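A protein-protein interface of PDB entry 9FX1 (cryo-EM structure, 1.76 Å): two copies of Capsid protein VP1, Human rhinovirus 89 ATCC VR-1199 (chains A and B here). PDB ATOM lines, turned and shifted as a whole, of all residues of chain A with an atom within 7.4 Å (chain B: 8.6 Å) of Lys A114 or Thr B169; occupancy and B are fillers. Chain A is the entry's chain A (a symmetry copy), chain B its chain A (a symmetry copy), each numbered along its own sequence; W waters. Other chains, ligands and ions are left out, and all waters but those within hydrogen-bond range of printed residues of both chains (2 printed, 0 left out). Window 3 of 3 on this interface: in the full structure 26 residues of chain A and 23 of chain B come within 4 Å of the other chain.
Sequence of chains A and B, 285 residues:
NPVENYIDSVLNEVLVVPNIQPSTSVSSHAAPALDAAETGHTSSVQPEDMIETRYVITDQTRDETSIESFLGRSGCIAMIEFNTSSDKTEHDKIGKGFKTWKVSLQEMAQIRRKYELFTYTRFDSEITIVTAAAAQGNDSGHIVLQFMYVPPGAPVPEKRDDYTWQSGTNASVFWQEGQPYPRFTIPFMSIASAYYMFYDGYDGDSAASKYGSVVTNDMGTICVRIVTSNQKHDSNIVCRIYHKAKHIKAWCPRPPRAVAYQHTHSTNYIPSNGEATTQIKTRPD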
ATOM      1  N   SER A  69      -5.584  13.536  35.085  1.00  0.00           N
ATOM      2  CA  SER A  69      -4.334  13.254  34.373  1.00  0.00           C
ATOM      3  C   SER A  69      -4.277  11.830  33.819  1.00  0.00           C
ATOM      4  O   SER A  69      -3.840  11.617  32.692  1.00  0.00           O
ATOM      5  CB  SER A  69      -3.146  13.489  35.304  1.00  0.00           C
ATOM      6  OG  SER A  69      -1.964  13.017  34.703  1.00  0.00           O
ATOM      7  N   PHE A  70      -4.660  10.829  34.611  1.00  0.00           N
ATOM      8  CA  PHE A  70      -4.476   9.427  34.247  1.00  0.00           C
ATOM      9  C   PHE A  70      -5.392   8.985  33.097  1.00  0.00           C
ATOM     10  O   PHE A  70      -4.920   8.370  32.143  1.00  0.00           O
ATOM     11  CB  PHE A  70      -4.688   8.566  35.493  1.00  0.00           C
ATOM     12  CG  PHE A  70      -4.577   7.087  35.213  1.00  0.00           C
ATOM     13  CD1 PHE A  70      -3.349   6.538  34.804  1.00  0.00           C
ATOM     14  CD2 PHE A  70      -5.697   6.249  35.382  1.00  0.00           C
ATOM     15  CE1 PHE A  70      -3.234   5.155  34.587  1.00  0.00           C
ATOM     16  CE2 PHE A  70      -5.583   4.875  35.153  1.00  0.00           C
ATOM     17  CZ  PHE A  70      -4.348   4.322  34.769  1.00  0.00           C
ATOM     18  N   LEU A  71      -6.682   9.311  33.166  1.00  0.00           N
ATOM     19  CA  LEU A  71      -7.663   8.965  32.125  1.00  0.00           C
ATOM     20  C   LEU A  71      -7.822  10.049  31.043  1.00  0.00           C
ATOM     21  O   LEU A  71      -8.312   9.763  29.951  1.00  0.00           O
ATOM     22  CB  LEU A  71      -9.012   8.636  32.796  1.00  0.00           C
ATOM     23  CG  LEU A  71      -9.021   7.437  33.760  1.00  0.00           C
ATOM     24  CD1 LEU A  71     -10.449   7.149  34.212  1.00  0.00           C
ATOM     25  CD2 LEU A  71      -8.475   6.161  33.124  1.00  0.00           C
ATOM     26  N   GLY A  72      -7.398  11.286  31.303  1.00  0.00           N
ATOM     27  CA  GLY A  72      -7.578  12.436  30.412  1.00  0.00           C
ATOM     28  C   GLY A  72      -6.526  12.562  29.316  1.00  0.00           C
ATOM     29  O   GLY A  72      -6.013  13.648  29.068  1.00  0.00           O
ATOM     30  N   ARG A  73      -6.199  11.456  28.644  1.00  0.00           N
ATOM     31  CA  ARG A  73      -5.246  11.395  27.522  1.00  0.00           C
ATOM     32  C   ARG A  73      -5.894  10.662  26.353  1.00  0.00           C
ATOM     33  O   ARG A  73      -6.551   9.646  26.565  1.00  0.00           O
ATOM     34  CB  ARG A  73      -3.942  10.707  27.960  1.00  0.00           C
ATOM     35  CG  ARG A  73      -3.275  11.455  29.121  1.00  0.00           C
ATOM     36  CD  ARG A  73      -2.041  10.735  29.662  1.00  0.00           C
ATOM     37  NE  ARG A  73      -1.619  11.396  30.908  1.00  0.00           N
ATOM     38  CZ  ARG A  73      -0.635  12.257  31.072  1.00  0.00           C
ATOM     39  NH1 ARG A  73      -0.570  12.953  32.166  1.00  0.00           N
ATOM     40  NH2 ARG A  73       0.276  12.457  30.169  1.00  0.00           N
ATOM     41  N   SER A  74      -5.726  11.162  25.134  1.00  0.00           N
ATOM     42  CA  SER A  74      -6.358  10.556  23.956  1.00  0.00           C
ATOM     43  C   SER A  74      -5.741   9.195  23.645  1.00  0.00           C
ATOM     44  O   SER A  74      -4.538   9.105  23.412  1.00  0.00           O
ATOM     45  CB  SER A  74      -6.237  11.456  22.720  1.00  0.00           C
ATOM     46  OG  SER A  74      -6.890  12.685  22.943  1.00  0.00           O
ATOM     47  N   GLY A  75      -6.561   8.148  23.588  1.00  0.00           N
ATOM     48  CA  GLY A  75      -6.142   6.813  23.152  1.00  0.00           C
ATOM     49  C   GLY A  75      -7.072   6.250  22.084  1.00  0.00           C
ATOM     50  O   GLY A  75      -8.249   6.597  22.040  1.00  0.00           O
ATOM     51  N   MET A 108     -10.010  -1.832  22.403  1.00  0.00           N
ATOM     52  CA  MET A 108      -8.581  -1.535  22.509  1.00  0.00           C
ATOM     53  C   MET A 108      -8.136  -1.663  23.969  1.00  0.00           C
ATOM     54  O   MET A 108      -8.618  -0.941  24.850  1.00  0.00           O
ATOM     55  CB  MET A 108      -8.282  -0.134  21.956  1.00  0.00           C
ATOM     56  CG  MET A 108      -8.725   0.046  20.503  1.00  0.00           C
ATOM     57  SD  MET A 108      -7.726  -0.913  19.354  1.00  0.00           S
ATOM     58  CE  MET A 108      -9.012  -1.871  18.515  1.00  0.00           C
ATOM     59  N   ALA A 109      -7.205  -2.577  24.227  1.00  0.00           N
ATOM     60  CA  ALA A 109      -6.831  -2.991  25.577  1.00  0.00           C
ATOM     61  C   ALA A 109      -6.157  -1.882  26.389  1.00  0.00           C
ATOM     62  O   ALA A 109      -6.383  -1.802  27.594  1.00  0.00           O
ATOM     63  CB  ALA A 109      -5.923  -4.216  25.479  1.00  0.00           C
ATOM     64  N   GLN A 110      -5.368  -1.007  25.752  1.00  0.00           N
ATOM     65  CA  GLN A 110      -4.664   0.049  26.478  1.00  0.00           C
ATOM     66  C   GLN A 110      -5.642   0.985  27.198  1.00  0.00           C
ATOM     67  O   GLN A 110      -5.522   1.165  28.410  1.00  0.00           O
ATOM     68  CB  GLN A 110      -3.719   0.841  25.565  1.00  0.00           C
ATOM     69  CG  GLN A 110      -2.520   0.025  25.061  1.00  0.00           C
ATOM     70  CD  GLN A 110      -1.405   0.933  24.546  1.00  0.00           C
ATOM     71  OE1 GLN A 110      -1.641   2.016  24.038  1.00  0.00           O
ATOM     72  NE2 GLN A 110      -0.156   0.550  24.681  1.00  0.00           N
ATOM     73  N   ILE A 111      -6.634   1.527  26.491  1.00  0.00           N
ATOM     74  CA  ILE A 111      -7.707   2.324  27.101  1.00  0.00           C
ATOM     75  C   ILE A 111      -8.541   1.462  28.047  1.00  0.00           C
ATOM     76  O   ILE A 111      -8.707   1.824  29.208  1.00  0.00           O
ATOM     77  CB  ILE A 111      -8.569   2.996  26.003  1.00  0.00           C
ATOM     78  CG1 ILE A 111      -7.851   4.251  25.465  1.00  0.00           C
ATOM     79  CG2 ILE A 111      -9.997   3.341  26.468  1.00  0.00           C
ATOM     80  CD1 ILE A 111      -7.879   5.477  26.392  1.00  0.00           C
ATOM     81  N   ARG A 112      -9.006   0.292  27.601  1.00  0.00           N
ATOM     82  CA  ARG A 112      -9.948  -0.532  28.376  1.00  0.00           C
ATOM     83  C   ARG A 112      -9.421  -0.825  29.777  1.00  0.00           C
ATOM     84  O   ARG A 112     -10.111  -0.593  30.765  1.00  0.00           O
ATOM     85  CB  ARG A 112     -10.228  -1.828  27.610  1.00  0.00           C
ATOM     86  CG  ARG A 112     -11.239  -2.699  28.358  1.00  0.00           C
ATOM     87  CD  ARG A 112     -11.499  -3.973  27.567  1.00  0.00           C
ATOM     88  NE  ARG A 112     -12.443  -4.831  28.289  1.00  0.00           N
ATOM     89  CZ  ARG A 112     -12.889  -6.012  27.928  1.00  0.00           C
ATOM     90  NH1 ARG A 112     -13.588  -6.702  28.775  1.00  0.00           N
ATOM     91  NH2 ARG A 112     -12.641  -6.509  26.750  1.00  0.00           N
ATOM     92  N   ARG A 113      -8.168  -1.265  29.875  1.00  0.00           N
ATOM     93  CA  ARG A 113      -7.549  -1.627  31.154  1.00  0.00           C
ATOM     94  C   ARG A 113      -7.494  -0.463  32.139  1.00  0.00           C
ATOM     95  O   ARG A 113      -7.770  -0.663  33.319  1.00  0.00           O
ATOM     96  CB  ARG A 113      -6.169  -2.216  30.868  1.00  0.00           C
ATOM     97  CG  ARG A 113      -5.565  -2.818  32.142  1.00  0.00           C
ATOM     98  CD  ARG A 113      -4.346  -3.635  31.743  1.00  0.00           C
ATOM     99  NE  ARG A 113      -3.757  -4.341  32.892  1.00  0.00           N
ATOM    100  CZ  ARG A 113      -2.766  -3.933  33.649  1.00  0.00           C
ATOM    101  NH1 ARG A 113      -2.195  -4.782  34.441  1.00  0.00           N
ATOM    102  NH2 ARG A 113      -2.334  -2.709  33.622  1.00  0.00           N
ATOM    103  N   LYS A 114      -7.201   0.744  31.651  1.00  0.00           N
ATOM    104  CA  LYS A 114      -7.133   1.958  32.477  1.00  0.00           C
ATOM    105  C   LYS A 114      -8.498   2.311  33.057  1.00  0.00           C
ATOM    106  O   LYS A 114      -8.608   2.513  34.256  1.00  0.00           O
ATOM    107  CB  LYS A 114      -6.562   3.133  31.667  1.00  0.00           C
ATOM    108  CG  LYS A 114      -5.079   2.916  31.331  1.00  0.00           C
ATOM    109  CD  LYS A 114      -4.514   4.021  30.428  1.00  0.00           C
ATOM    110  CE  LYS A 114      -4.543   5.384  31.125  1.00  0.00           C
ATOM    111  NZ  LYS A 114      -3.948   6.449  30.274  1.00  0.00           N
ATOM    112  N   TYR A 115      -9.545   2.344  32.239  1.00  0.00           N
ATOM    113  CA  TYR A 115     -10.885   2.682  32.737  1.00  0.00           C
ATOM    114  C   TYR A 115     -11.422   1.573  33.655  1.00  0.00           C
ATOM    115  O   TYR A 115     -12.051   1.846  34.667  1.00  0.00           O
ATOM    116  CB  TYR A 115     -11.836   2.969  31.570  1.00  0.00           C
ATOM    117  CG  TYR A 115     -11.591   4.299  30.881  1.00  0.00           C
ATOM    118  CD1 TYR A 115     -10.410   4.520  30.155  1.00  0.00           C
ATOM    119  CD2 TYR A 115     -12.544   5.333  30.969  1.00  0.00           C
ATOM    120  CE1 TYR A 115     -10.173   5.744  29.510  1.00  0.00           C
ATOM    121  CE2 TYR A 115     -12.321   6.558  30.306  1.00  0.00           C
ATOM    122  CZ  TYR A 115     -11.141   6.759  29.565  1.00  0.00           C
ATOM    123  OH  TYR A 115     -10.907   7.929  28.913  1.00  0.00           O
ATOM    124  N   GLU A 116     -11.100   0.314  33.369  1.00  0.00           N
ATOM    125  CA  GLU A 116     -11.461  -0.819  34.219  1.00  0.00           C
ATOM    126  C   GLU A 116     -10.710  -0.911  35.560  1.00  0.00           C
ATOM    127  O   GLU A 116     -11.019  -1.785  36.365  1.00  0.00           O
ATOM    128  CB  GLU A 116     -11.280  -2.113  33.438  1.00  0.00           C
ATOM    129  CG  GLU A 116     -12.416  -2.329  32.429  1.00  0.00           C
ATOM    130  CD  GLU A 116     -12.326  -3.710  31.772  1.00  0.00           C
ATOM    131  OE1 GLU A 116     -11.450  -4.512  32.175  1.00  0.00           O
ATOM    132  OE2 GLU A 116     -13.112  -3.984  30.840  1.00  0.00           O
ATOM    133  N   LEU A 117      -9.772  -0.012  35.867  1.00  0.00           N
ATOM    134  CA  LEU A 117      -9.317   0.171  37.254  1.00  0.00           C
ATOM    135  C   LEU A 117     -10.425   0.700  38.175  1.00  0.00           C
ATOM    136  O   LEU A 117     -10.240   0.728  39.384  1.00  0.00           O
ATOM    137  CB  LEU A 117      -8.109   1.121  37.293  1.00  0.00           C
ATOM    138  CG  LEU A 117      -6.791   0.431  36.913  1.00  0.00           C
ATOM    139  CD1 LEU A 117      -5.736   1.488  36.610  1.00  0.00           C
ATOM    140  CD2 LEU A 117      -6.291  -0.444  38.066  1.00  0.00           C
ATOM    141  N   PHE A 118     -11.572   1.099  37.631  1.00  0.00           N
ATOM    142  CA  PHE A 118     -12.697   1.661  38.365  1.00  0.00           C
ATOM    143  C   PHE A 118     -13.970   0.890  38.048  1.00  0.00           C
ATOM    144  O   PHE A 118     -14.110   0.304  36.978  1.00  0.00           O
ATOM    145  CB  PHE A 118     -12.830   3.147  38.039  1.00  0.00           C
ATOM    146  CG  PHE A 118     -11.496   3.855  38.151  1.00  0.00           C
ATOM    147  CD1 PHE A 118     -10.952   4.138  39.417  1.00  0.00           C
ATOM    148  CD2 PHE A 118     -10.753   4.111  36.987  1.00  0.00           C
ATOM    149  CE1 PHE A 118      -9.654   4.672  39.511  1.00  0.00           C
ATOM    150  CE2 PHE A 118      -9.456   4.636  37.083  1.00  0.00           C
ATOM    151  CZ  PHE A 118      -8.905   4.904  38.347  1.00  0.00           C
ATOM    152  N   THR A 121     -17.503   5.080  36.179  1.00  0.00           N
ATOM    153  CA  THR A 121     -16.817   6.275  35.687  1.00  0.00           C
ATOM    154  C   THR A 121     -17.834   7.238  35.094  1.00  0.00           C
ATOM    155  O   THR A 121     -18.844   6.828  34.541  1.00  0.00           O
ATOM    156  CB  THR A 121     -15.715   5.931  34.673  1.00  0.00           C
ATOM    157  OG1 THR A 121     -16.258   5.211  33.593  1.00  0.00           O
ATOM    158  CG2 THR A 121     -14.570   5.105  35.261  1.00  0.00           C
ATOM    159  N   MET A 197     -18.342   0.251  34.266  1.00  0.00           N
ATOM    160  CA  MET A 197     -17.236  -0.543  33.707  1.00  0.00           C
ATOM    161  C   MET A 197     -17.496  -2.048  33.870  1.00  0.00           C
ATOM    162  O   MET A 197     -17.091  -2.851  33.038  1.00  0.00           O
ATOM    163  CB  MET A 197     -15.905  -0.168  34.369  1.00  0.00           C
ATOM    164  CG  MET A 197     -15.554   1.319  34.260  1.00  0.00           C
ATOM    165  SD  MET A 197     -15.700   2.058  32.609  1.00  0.00           S
ATOM    166  CE  MET A 197     -14.717   0.916  31.605  1.00  0.00           C
ATOM    167  N   PRO A 256      -6.288  -4.326  38.638  1.00  0.00           N
ATOM    168  CA  PRO A 256      -6.132  -4.234  37.194  1.00  0.00           C
ATOM    169  C   PRO A 256      -6.286  -5.606  36.541  1.00  0.00           C
ATOM    170  O   PRO A 256      -5.963  -6.637  37.137  1.00  0.00           O
ATOM    171  CB  PRO A 256      -4.730  -3.677  36.953  1.00  0.00           C
ATOM    172  CG  PRO A 256      -3.978  -4.039  38.227  1.00  0.00           C
ATOM    173  CD  PRO A 256      -5.042  -4.040  39.318  1.00  0.00           C
ATOM    174  N   ARG A 257      -6.707  -5.616  35.277  1.00  0.00           N
ATOM    175  CA  ARG A 257      -6.723  -6.817  34.438  1.00  0.00           C
ATOM    176  C   ARG A 257      -5.338  -7.475  34.458  1.00  0.00           C
ATOM    177  O   ARG A 257      -4.352  -6.823  34.116  1.00  0.00           O
ATOM    178  CB  ARG A 257      -7.137  -6.411  33.014  1.00  0.00           C
ATOM    179  CG  ARG A 257      -7.323  -7.613  32.093  1.00  0.00           C
ATOM    180  CD  ARG A 257      -8.541  -8.459  32.479  1.00  0.00           C
ATOM    181  NE  ARG A 257      -8.695  -9.585  31.551  1.00  0.00           N
ATOM    182  CZ  ARG A 257      -9.734 -10.387  31.444  1.00  0.00           C
ATOM    183  NH1 ARG A 257      -9.741 -11.332  30.551  1.00  0.00           N
ATOM    184  NH2 ARG A 257     -10.775 -10.282  32.219  1.00  0.00           N
ATOM    185  N   TYR A 261      -7.437  -9.794  27.631  1.00  0.00           N
ATOM    186  CA  TYR A 261      -8.853  -9.742  27.265  1.00  0.00           C
ATOM    187  C   TYR A 261      -9.147 -10.742  26.143  1.00  0.00           C
ATOM    188  O   TYR A 261      -8.309 -10.982  25.279  1.00  0.00           O
ATOM    189  CB  TYR A 261      -9.259  -8.328  26.844  1.00  0.00           C
ATOM    190  CG  TYR A 261      -9.207  -7.327  27.971  1.00  0.00           C
ATOM    191  CD1 TYR A 261     -10.108  -7.437  29.045  1.00  0.00           C
ATOM    192  CD2 TYR A 261      -8.289  -6.266  27.923  1.00  0.00           C
ATOM    193  CE1 TYR A 261     -10.097  -6.480  30.070  1.00  0.00           C
ATOM    194  CE2 TYR A 261      -8.264  -5.312  28.953  1.00  0.00           C
ATOM    195  CZ  TYR A 261      -9.175  -5.416  30.023  1.00  0.00           C
ATOM    196  OH  TYR A 261      -9.174  -4.483  31.004  1.00  0.00           O
ATOM    197  N   MET B 148       5.211   8.829  18.245  1.00  0.00           N
ATOM    198  CA  MET B 148       4.877   8.437  19.603  1.00  0.00           C
ATOM    199  C   MET B 148       6.131   8.501  20.464  1.00  0.00           C
ATOM    200  O   MET B 148       7.132   7.866  20.141  1.00  0.00           O
ATOM    201  CB  MET B 148       4.255   7.038  19.584  1.00  0.00           C
ATOM    202  CG  MET B 148       3.853   6.589  20.990  1.00  0.00           C
ATOM    203  SD  MET B 148       2.848   5.082  21.016  1.00  0.00           S
ATOM    204  CE  MET B 148       3.988   3.907  20.231  1.00  0.00           C
ATOM    205  N   TYR B 149       6.090   9.260  21.553  1.00  0.00           N
ATOM    206  CA  TYR B 149       7.155   9.209  22.541  1.00  0.00           C
ATOM    207  C   TYR B 149       6.921   8.026  23.478  1.00  0.00           C
ATOM    208  O   TYR B 149       5.901   7.964  24.158  1.00  0.00           O
ATOM    209  CB  TYR B 149       7.250  10.515  23.325  1.00  0.00           C
ATOM    210  CG  TYR B 149       8.311  10.414  24.396  1.00  0.00           C
ATOM    211  CD1 TYR B 149       9.652  10.240  24.017  1.00  0.00           C
ATOM    212  CD2 TYR B 149       7.948  10.391  25.755  1.00  0.00           C
ATOM    213  CE1 TYR B 149      10.643  10.089  25.001  1.00  0.00           C
ATOM    214  CE2 TYR B 149       8.940  10.244  26.742  1.00  0.00           C
ATOM    215  CZ  TYR B 149      10.285  10.095  26.364  1.00  0.00           C
ATOM    216  OH  TYR B 149      11.233   9.928  27.315  1.00  0.00           O
ATOM    217  N   VAL B 150       7.869   7.099  23.515  1.00  0.00           N
ATOM    218  CA  VAL B 150       7.842   5.915  24.378  1.00  0.00           C
ATOM    219  C   VAL B 150       8.828   6.140  25.533  1.00  0.00           C
ATOM    220  O   VAL B 150      10.040   6.042  25.307  1.00  0.00           O
ATOM    221  CB  VAL B 150       8.174   4.653  23.555  1.00  0.00           C
ATOM    222  CG1 VAL B 150       8.111   3.387  24.413  1.00  0.00           C
ATOM    223  CG2 VAL B 150       7.175   4.468  22.405  1.00  0.00           C
ATOM    224  N   PRO B 151       8.361   6.484  26.751  1.00  0.00           N
ATOM    225  CA  PRO B 151       9.241   6.662  27.905  1.00  0.00           C
ATOM    226  C   PRO B 151      10.002   5.369  28.236  1.00  0.00           C
ATOM    227  O   PRO B 151       9.553   4.286  27.861  1.00  0.00           O
ATOM    228  CB  PRO B 151       8.334   7.071  29.077  1.00  0.00           C
ATOM    229  CG  PRO B 151       7.033   7.527  28.421  1.00  0.00           C
ATOM    230  CD  PRO B 151       6.977   6.710  27.137  1.00  0.00           C
ATOM    231  N   ALA B 154       8.249   1.653  28.877  1.00  0.00           N
ATOM    232  CA  ALA B 154       7.050   1.437  28.069  1.00  0.00           C
ATOM    233  C   ALA B 154       7.372   0.530  26.859  1.00  0.00           C
ATOM    234  O   ALA B 154       8.494   0.571  26.343  1.00  0.00           O
ATOM    235  CB  ALA B 154       6.482   2.796  27.658  1.00  0.00           C
ATOM    236  N   THR B 164       0.787  -1.087  20.628  1.00  0.00           N
ATOM    237  CA  THR B 164       1.451   0.046  21.294  1.00  0.00           C
ATOM    238  C   THR B 164       1.071   1.390  20.666  1.00  0.00           C
ATOM    239  O   THR B 164       0.956   2.385  21.377  1.00  0.00           O
ATOM    240  CB  THR B 164       2.974  -0.123  21.282  1.00  0.00           C
ATOM    241  OG1 THR B 164       3.437  -0.142  19.961  1.00  0.00           O
ATOM    242  CG2 THR B 164       3.431  -1.426  21.926  1.00  0.00           C
ATOM    243  N   TRP B 165       0.780   1.425  19.363  1.00  0.00           N
ATOM    244  CA  TRP B 165       0.369   2.645  18.663  1.00  0.00           C
ATOM    245  C   TRP B 165      -1.011   3.181  19.072  1.00  0.00           C
ATOM    246  O   TRP B 165      -1.336   4.317  18.730  1.00  0.00           O
ATOM    247  CB  TRP B 165       0.406   2.409  17.159  1.00  0.00           C
ATOM    248  CG  TRP B 165       1.740   2.016  16.624  1.00  0.00           C
ATOM    249  CD1 TRP B 165       2.082   0.782  16.204  1.00  0.00           C
ATOM    250  CD2 TRP B 165       2.917   2.852  16.419  1.00  0.00           C
ATOM    251  NE1 TRP B 165       3.380   0.792  15.739  1.00  0.00           N
ATOM    252  CE2 TRP B 165       3.939   2.043  15.838  1.00  0.00           C
ATOM    253  CE3 TRP B 165       3.219   4.213  16.635  1.00  0.00           C
ATOM    254  CZ2 TRP B 165       5.190   2.556  15.487  1.00  0.00           C
ATOM    255  CZ3 TRP B 165       4.477   4.740  16.284  1.00  0.00           C
ATOM    256  CH2 TRP B 165       5.457   3.916  15.704  1.00  0.00           C
ATOM    257  N   GLN B 166      -1.811   2.420  19.832  1.00  0.00           N
ATOM    258  CA  GLN B 166      -3.061   2.928  20.417  1.00  0.00           C
ATOM    259  C   GLN B 166      -2.826   4.173  21.278  1.00  0.00           C
ATOM    260  O   GLN B 166      -3.711   5.019  21.404  1.00  0.00           O
ATOM    261  CB  GLN B 166      -3.707   1.851  21.298  1.00  0.00           C
ATOM    262  CG  GLN B 166      -4.228   0.645  20.502  1.00  0.00           C
ATOM    263  CD  GLN B 166      -4.642  -0.515  21.409  1.00  0.00           C
ATOM    264  OE1 GLN B 166      -4.855  -0.374  22.605  1.00  0.00           O
ATOM    265  NE2 GLN B 166      -4.805  -1.702  20.873  1.00  0.00           N
ATOM    266  N   SER B 167      -1.624   4.304  21.852  1.00  0.00           N
ATOM    267  CA  SER B 167      -1.168   5.496  22.571  1.00  0.00           C
ATOM    268  C   SER B 167      -2.097   5.899  23.726  1.00  0.00           C
ATOM    269  O   SER B 167      -2.322   7.082  23.969  1.00  0.00           O
ATOM    270  CB  SER B 167      -0.917   6.633  21.575  1.00  0.00           C
ATOM    271  OG  SER B 167      -0.060   7.611  22.122  1.00  0.00           O
ATOM    272  N   GLY B 168      -2.652   4.918  24.444  1.00  0.00           N
ATOM    273  CA  GLY B 168      -3.601   5.164  25.540  1.00  0.00           C
ATOM    274  C   GLY B 168      -3.021   5.972  26.708  1.00  0.00           C
ATOM    275  O   GLY B 168      -3.767   6.599  27.456  1.00  0.00           O
ATOM    276  N   THR B 169      -1.691   5.993  26.847  1.00  0.00           N
ATOM    277  CA  THR B 169      -0.977   6.746  27.897  1.00  0.00           C
ATOM    278  C   THR B 169       0.231   7.527  27.364  1.00  0.00           C
ATOM    279  O   THR B 169       0.477   8.646  27.813  1.00  0.00           O
ATOM    280  CB  THR B 169      -0.565   5.796  29.035  1.00  0.00           C
ATOM    281  OG1 THR B 169      -1.682   5.072  29.504  1.00  0.00           O
ATOM    282  CG2 THR B 169       0.022   6.523  30.239  1.00  0.00           C
ATOM    283  N   ASN B 170       0.964   6.994  26.380  1.00  0.00           N
ATOM    284  CA  ASN B 170       2.045   7.725  25.710  1.00  0.00           C
ATOM    285  C   ASN B 170       1.532   8.991  25.003  1.00  0.00           C
ATOM    286  O   ASN B 170       0.421   9.017  24.473  1.00  0.00           O
ATOM    287  CB  ASN B 170       2.734   6.830  24.667  1.00  0.00           C
ATOM    288  CG  ASN B 170       3.480   5.646  25.245  1.00  0.00           C
ATOM    289  OD1 ASN B 170       3.774   5.558  26.426  1.00  0.00           O
ATOM    290  ND2 ASN B 170       3.766   4.689  24.402  1.00  0.00           N
ATOM    291  N   ALA B 171       2.377  10.018  24.916  1.00  0.00           N
ATOM    292  CA  ALA B 171       2.135  11.135  24.018  1.00  0.00           C
ATOM    293  C   ALA B 171       2.356  10.690  22.561  1.00  0.00           C
ATOM    294  O   ALA B 171       3.424  10.186  22.218  1.00  0.00           O
ATOM    295  CB  ALA B 171       3.060  12.294  24.397  1.00  0.00           C
ATOM    296  N   SER B 172       1.368  10.929  21.702  1.00  0.00           N
ATOM    297  CA  SER B 172       1.529  10.863  20.245  1.00  0.00           C
ATOM    298  C   SER B 172       1.175  12.203  19.613  1.00  0.00           C
ATOM    299  O   SER B 172       0.274  12.895  20.086  1.00  0.00           O
ATOM    300  CB  SER B 172       0.666   9.780  19.591  1.00  0.00           C
ATOM    301  OG  SER B 172       1.142   8.484  19.864  1.00  0.00           O
HETATM  302  O   HOH W   1      -6.378   2.048  23.494  1.00  0.00           O
HETATM  303  O   HOH W   2      -4.392  -2.114  18.008  1.00  0.00           O
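Of the printed residues of chain B, Lys A114 touches Gly B168 and Thr B169.
Gly B168 touches just these residues of chain A: Gly A75 (3.9 Å), Gln A110 (3.1 Å) and Lys A114 (2.8 Å).
Of the printed residues of chain B, Arg A73 touches Thr B169.
Printed residues of chain A within 4 Å of Thr B164: Gln A110 (3.7 Å).
Of the printed residues of chain B, Ala A109 touches Gln B166 (3.6 Å).
Of the printed residues of chain A, Gln B166 touches Gly A75, Met A108, Ala A109 and Gln A110.
The nearest residue of chain B that does not touch Lys A114 is Asn B170 (6.3 Å).
Thr B169 touches Arg A73 (O to CD, 3.8 Å).
Gln B166 touches Gly A75.
Ser B167 touches Gly A75.
Gly A75 touches Gly B168.
N of Ala A109 touches OE1 of Gln B166, at 3.6 Å.
Thr B164 touches Gln A110.
The side-chain amide nitrogen (NE2) of Gln B166 lies within hydrogen-bond range of the side-chain sulfur (SD) of Met A108 (3.4 Å).
OE1 of Gln B166 lies within hydrogen-bond range of N of Gln A110 (3.3 Å).
The backbone NH (N) of Ser B167 is in hydrogen-bond range of the side-chain amide oxygen (OE1) of Gln A110 (3.2 Å).
The side-chain amide oxygen (OE1) of Gln A110 is in hydrogen-bond range of the backbone NH (N) of Gly B168 (3.1 Å).
NZ of Lys A114 sits at hydrogen-bond distance from O of Gly B168 (2.8 Å).
NZ of Lys A114 sits at hydrogen-bond distance from OG1 of Thr B169 (2.8 Å).
The backbone carbonyl oxygen of Ser A74 sits close to the backbone carbonyl oxygen of Ser B167, at 3.1 Å.
The side-chain hydroxyl (OG) of Ser B167 sits at hydrogen-bond distance from the backbone carbonyl oxygen (O) of Asn B170 (2.8 Å).
OG of Ser B167 sits at hydrogen-bond distance from OG of Ser B172 (2.7 Å).
The backbone carbonyl oxygen (O) of Ser A69 sits at hydrogen-bond distance from the guanidinium group (NE) of Arg A73 (2.9 Å).
The backbone carbonyl oxygen (O) of Phe A70 lies within hydrogen-bond range of the side-chain amino group (NZ) of Lys A114, 2.9 Å away.
Water W2 bridges the side-chain amide nitrogen of Gln B166 (2.9 Å) and the side-chain sulfur of Met A108 (3.8 Å).
Water W1 bridges the side-chain amide oxygen (OE1) of Gln B166 (3.0 Å) and the backbone NH (N) of Ile A111 (3.1 Å).
No position is printed for both chains.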
